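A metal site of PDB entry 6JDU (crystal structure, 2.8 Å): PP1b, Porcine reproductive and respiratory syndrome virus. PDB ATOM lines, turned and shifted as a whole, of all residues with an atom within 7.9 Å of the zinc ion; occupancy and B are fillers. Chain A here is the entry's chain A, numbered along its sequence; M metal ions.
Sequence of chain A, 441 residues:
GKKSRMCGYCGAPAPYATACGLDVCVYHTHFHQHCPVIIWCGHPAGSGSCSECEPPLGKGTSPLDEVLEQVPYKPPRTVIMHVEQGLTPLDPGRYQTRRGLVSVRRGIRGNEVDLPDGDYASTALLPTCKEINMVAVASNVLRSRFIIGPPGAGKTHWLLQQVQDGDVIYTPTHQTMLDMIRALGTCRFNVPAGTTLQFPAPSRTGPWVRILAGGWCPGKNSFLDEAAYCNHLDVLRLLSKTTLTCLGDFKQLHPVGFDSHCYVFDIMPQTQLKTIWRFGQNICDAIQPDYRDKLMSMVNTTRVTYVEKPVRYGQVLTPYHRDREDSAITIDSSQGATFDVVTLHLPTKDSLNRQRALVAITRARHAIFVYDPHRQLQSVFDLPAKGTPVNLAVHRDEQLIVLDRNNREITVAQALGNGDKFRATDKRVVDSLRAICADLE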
ATOM      1  N   MET A   6     -24.613 -11.790  -3.641  1.00  0.00           N
ATOM      2  CA  MET A   6     -24.240 -11.759  -5.056  1.00  0.00           C
ATOM      3  C   MET A   6     -24.893 -10.587  -5.770  1.00  0.00           C
ATOM      4  O   MET A   6     -26.030 -10.203  -5.450  1.00  0.00           O
ATOM      5  CB  MET A   6     -24.660 -13.059  -5.751  1.00  0.00           C
ATOM      6  CG  MET A   6     -24.102 -14.351  -5.152  1.00  0.00           C
ATOM      7  SD  MET A   6     -22.298 -14.495  -5.236  1.00  0.00           S
ATOM      8  CE  MET A   6     -21.784 -13.754  -3.686  1.00  0.00           C
ATOM      9  N   CYS A   7     -24.186 -10.033  -6.753  1.00  0.00           N
ATOM     10  CA  CYS A   7     -24.677  -8.949  -7.608  1.00  0.00           C
ATOM     11  C   CYS A   7     -25.981  -9.321  -8.331  1.00  0.00           C
ATOM     12  O   CYS A   7     -26.185 -10.474  -8.701  1.00  0.00           O
ATOM     13  CB  CYS A   7     -23.599  -8.549  -8.617  1.00  0.00           C
ATOM     14  SG  CYS A   7     -24.041  -7.241  -9.798  1.00  0.00           S
ATOM     15  N   GLY A   8     -26.853  -8.341  -8.530  1.00  0.00           N
ATOM     16  CA  GLY A   8     -28.121  -8.545  -9.215  1.00  0.00           C
ATOM     17  C   GLY A   8     -28.003  -8.729 -10.716  1.00  0.00           C
ATOM     18  O   GLY A   8     -28.794  -9.469 -11.315  1.00  0.00           O
ATOM     19  N   TYR A   9     -27.034  -8.047 -11.335  1.00  0.00           N
ATOM     20  CA  TYR A   9     -26.813  -8.106 -12.782  1.00  0.00           C
ATOM     21  C   TYR A   9     -25.972  -9.329 -13.162  1.00  0.00           C
ATOM     22  O   TYR A   9     -26.431 -10.215 -13.882  1.00  0.00           O
ATOM     23  CB  TYR A   9     -26.114  -6.834 -13.291  1.00  0.00           C
ATOM     24  CG  TYR A   9     -26.868  -5.549 -13.073  1.00  0.00           C
ATOM     25  CD1 TYR A   9     -28.008  -5.251 -13.837  1.00  0.00           C
ATOM     26  CD2 TYR A   9     -26.447  -4.607 -12.144  1.00  0.00           C
ATOM     27  CE1 TYR A   9     -28.704  -4.067 -13.657  1.00  0.00           C
ATOM     28  CE2 TYR A   9     -27.128  -3.416 -11.961  1.00  0.00           C
ATOM     29  CZ  TYR A   9     -28.262  -3.148 -12.723  1.00  0.00           C
ATOM     30  OH  TYR A   9     -28.937  -1.970 -12.542  1.00  0.00           O
ATOM     31  N   CYS A  10     -24.732  -9.345 -12.650  1.00  0.00           N
ATOM     32  CA  CYS A  10     -23.755 -10.399 -12.910  1.00  0.00           C
ATOM     33  C   CYS A  10     -23.693 -11.287 -11.662  1.00  0.00           C
ATOM     34  O   CYS A  10     -24.428 -11.059 -10.701  1.00  0.00           O
ATOM     35  CB  CYS A  10     -22.388  -9.773 -13.184  1.00  0.00           C
ATOM     36  SG  CYS A  10     -21.696  -8.771 -11.836  1.00  0.00           S
ATOM     37  N   GLY A  11     -22.826 -12.294 -11.677  1.00  0.00           N
ATOM     38  CA  GLY A  11     -22.657 -13.150 -10.507  1.00  0.00           C
ATOM     39  C   GLY A  11     -21.917 -12.546  -9.326  1.00  0.00           C
ATOM     40  O   GLY A  11     -22.143 -12.958  -8.186  1.00  0.00           O
ATOM     41  N   ALA A  12     -21.078 -11.537  -9.588  1.00  0.00           N
ATOM     42  CA  ALA A  12     -19.962 -11.170  -8.712  1.00  0.00           C
ATOM     43  C   ALA A  12     -20.345 -10.712  -7.313  1.00  0.00           C
ATOM     44  O   ALA A  12     -21.483 -10.287  -7.098  1.00  0.00           O
ATOM     45  CB  ALA A  12     -19.114 -10.091  -9.390  1.00  0.00           C
ATOM     46  N   PRO A  13     -19.395 -10.795  -6.345  1.00  0.00           N
ATOM     47  CA  PRO A  13     -19.638 -10.313  -4.974  1.00  0.00           C
ATOM     48  C   PRO A  13     -20.097  -8.848  -4.908  1.00  0.00           C
ATOM     49  O   PRO A  13     -19.613  -8.012  -5.664  1.00  0.00           O
ATOM     50  CB  PRO A  13     -18.271 -10.473  -4.300  1.00  0.00           C
ATOM     51  CG  PRO A  13     -17.655 -11.616  -5.012  1.00  0.00           C
ATOM     52  CD  PRO A  13     -18.083 -11.467  -6.446  1.00  0.00           C
ATOM     53  N   ALA A  14     -21.041  -8.573  -4.005  1.00  0.00           N
ATOM     54  CA  ALA A  14     -21.768  -7.299  -3.967  1.00  0.00           C
ATOM     55  C   ALA A  14     -21.717  -6.668  -2.571  1.00  0.00           C
ATOM     56  O   ALA A  14     -22.551  -6.973  -1.719  1.00  0.00           O
ATOM     57  CB  ALA A  14     -23.207  -7.508  -4.401  1.00  0.00           C
ATOM     58  N   ASP A  23     -28.729  -5.709  -5.101  1.00  0.00           N
ATOM     59  CA  ASP A  23     -27.320  -5.842  -4.727  1.00  0.00           C
ATOM     60  C   ASP A  23     -26.460  -5.663  -5.963  1.00  0.00           C
ATOM     61  O   ASP A  23     -26.807  -6.158  -7.033  1.00  0.00           O
ATOM     62  CB  ASP A  23     -27.032  -7.229  -4.132  1.00  0.00           C
ATOM     63  CG  ASP A  23     -27.777  -7.477  -2.828  1.00  0.00           C
ATOM     64  OD1 ASP A  23     -27.947  -6.518  -2.042  1.00  0.00           O
ATOM     65  OD2 ASP A  23     -28.182  -8.629  -2.576  1.00  0.00           O
ATOM     66  N   VAL A  24     -25.340  -4.958  -5.819  1.00  0.00           N
ATOM     67  CA  VAL A  24     -24.453  -4.674  -6.947  1.00  0.00           C
ATOM     68  C   VAL A  24     -22.981  -4.849  -6.574  1.00  0.00           C
ATOM     69  O   VAL A  24     -22.569  -4.529  -5.466  1.00  0.00           O
ATOM     70  CB  VAL A  24     -24.682  -3.256  -7.519  1.00  0.00           C
ATOM     71  CG1 VAL A  24     -26.050  -3.152  -8.155  1.00  0.00           C
ATOM     72  CG2 VAL A  24     -24.517  -2.174  -6.452  1.00  0.00           C
ATOM     73  N   CYS A  25     -22.204  -5.359  -7.533  1.00  0.00           N
ATOM     74  CA  CYS A  25     -20.745  -5.403  -7.447  1.00  0.00           C
ATOM     75  C   CYS A  25     -20.189  -3.992  -7.685  1.00  0.00           C
ATOM     76  O   CYS A  25     -20.942  -3.095  -8.087  1.00  0.00           O
ATOM     77  CB  CYS A  25     -20.187  -6.372  -8.485  1.00  0.00           C
ATOM     78  SG  CYS A  25     -20.497  -5.896 -10.203  1.00  0.00           S
ATOM     79  N   VAL A  26     -18.890  -3.796  -7.456  1.00  0.00           N
ATOM     80  CA  VAL A  26     -18.311  -2.451  -7.531  1.00  0.00           C
ATOM     81  C   VAL A  26     -18.401  -1.885  -8.953  1.00  0.00           C
ATOM     82  O   VAL A  26     -18.650  -0.684  -9.116  1.00  0.00           O
ATOM     83  CB  VAL A  26     -16.855  -2.350  -6.976  1.00  0.00           C
ATOM     84  CG1 VAL A  26     -16.784  -2.886  -5.554  1.00  0.00           C
ATOM     85  CG2 VAL A  26     -15.859  -3.059  -7.882  1.00  0.00           C
ATOM     86  N   TYR A  27     -18.229  -2.741  -9.959  1.00  0.00           N
ATOM     87  CA  TYR A  27     -18.405  -2.338 -11.358  1.00  0.00           C
ATOM     88  C   TYR A  27     -19.803  -1.775 -11.624  1.00  0.00           C
ATOM     89  O   TYR A  27     -19.946  -0.715 -12.227  1.00  0.00           O
ATOM     90  CB  TYR A  27     -18.130  -3.503 -12.313  1.00  0.00           C
ATOM     91  CG  TYR A  27     -18.334  -3.156 -13.779  1.00  0.00           C
ATOM     92  CD1 TYR A  27     -17.427  -2.328 -14.451  1.00  0.00           C
ATOM     93  CD2 TYR A  27     -19.442  -3.630 -14.485  1.00  0.00           C
ATOM     94  CE1 TYR A  27     -17.611  -1.988 -15.779  1.00  0.00           C
ATOM     95  CE2 TYR A  27     -19.650  -3.292 -15.819  1.00  0.00           C
ATOM     96  CZ  TYR A  27     -18.731  -2.469 -16.470  1.00  0.00           C
ATOM     97  OH  TYR A  27     -18.926  -2.138 -17.784  1.00  0.00           O
ATOM     98  N   HIS A  28     -20.823  -2.481 -11.143  1.00  0.00           N
ATOM     99  CA  HIS A  28     -22.218  -2.135 -11.430  1.00  0.00           C
ATOM    100  C   HIS A  28     -22.769  -0.956 -10.618  1.00  0.00           C
ATOM    101  O   HIS A  28     -23.881  -0.483 -10.914  1.00  0.00           O
ATOM    102  CB  HIS A  28     -23.115  -3.370 -11.340  1.00  0.00           C
ATOM    103  CG  HIS A  28     -23.043  -4.243 -12.561  1.00  0.00           C
ATOM    104  ND1 HIS A  28     -22.498  -5.518 -12.536  1.00  0.00           N
ATOM    105  CD2 HIS A  28     -23.404  -4.011 -13.840  1.00  0.00           C
ATOM    106  CE1 HIS A  28     -22.555  -6.024 -13.756  1.00  0.00           C
ATOM    107  NE2 HIS A  28     -23.097  -5.130 -14.562  1.00  0.00           N
ATOM    108  N   THR A  29     -22.019  -0.463  -9.632  1.00  0.00           N
ATOM    109  CA  THR A  29     -22.400   0.748  -8.903  1.00  0.00           C
ATOM    110  C   THR A  29     -22.549   1.985  -9.804  1.00  0.00           C
ATOM    111  O   THR A  29     -23.243   2.923  -9.437  1.00  0.00           O
ATOM    112  CB  THR A  29     -21.396   1.105  -7.773  1.00  0.00           C
ATOM    113  OG1 THR A  29     -20.081   1.279  -8.312  1.00  0.00           O
ATOM    114  CG2 THR A  29     -21.372   0.030  -6.687  1.00  0.00           C
ATOM    115  N   THR A  61     -26.346  -1.875 -18.400  1.00  0.00           N
ATOM    116  CA  THR A  61     -25.744  -3.066 -19.010  1.00  0.00           C
ATOM    117  C   THR A  61     -26.698  -4.276 -19.036  1.00  0.00           C
ATOM    118  O   THR A  61     -26.273  -5.389 -19.352  1.00  0.00           O
ATOM    119  CB  THR A  61     -24.445  -3.462 -18.256  1.00  0.00           C
ATOM    120  OG1 THR A  61     -24.761  -3.835 -16.900  1.00  0.00           O
ATOM    121  CG2 THR A  61     -23.454  -2.303 -18.243  1.00  0.00           C
HETATM  122 ZN    ZN M   1     -22.336  -6.866 -11.155  1.00  0.00          ZN
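Within 4 Å of the zinc ion: Cys 7, Cys 10, Cys 25 and His 28.
The nearest printed residue that does not touch the zinc ion is Tyr 9 (4.3 Å).
The side-chain sulfur (SG) of Cys 10 sits close to the backbone NH (N) of Ala 12, at 3.6 Å.
The side-chain hydroxyl (OG1) of Thr 61 sits at hydrogen-bond distance from a ring nitrogen (NE2) of His 28 (3.1 Å).
The side-chain sulfur (SG) of Cys 7 lies close to the backbone NH (N) of Tyr 9 (3.5 Å).
The backbone NH (N) of Cys 7 lies within hydrogen-bond range of the backbone carbonyl oxygen (O) of Ala 12.
The zinc ion is bound by a ring nitrogen (ND1) of His 28 (1.9 Å), the side-chain sulfur (SG) of Cys 10 (2.1 Å), the side-chain sulfur (SG) of Cys 7 (2.2 Å) and the side-chain sulfur (SG) of Cys 25 (2.3 Å).
The zinc ion has four donor atoms within binding distance.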
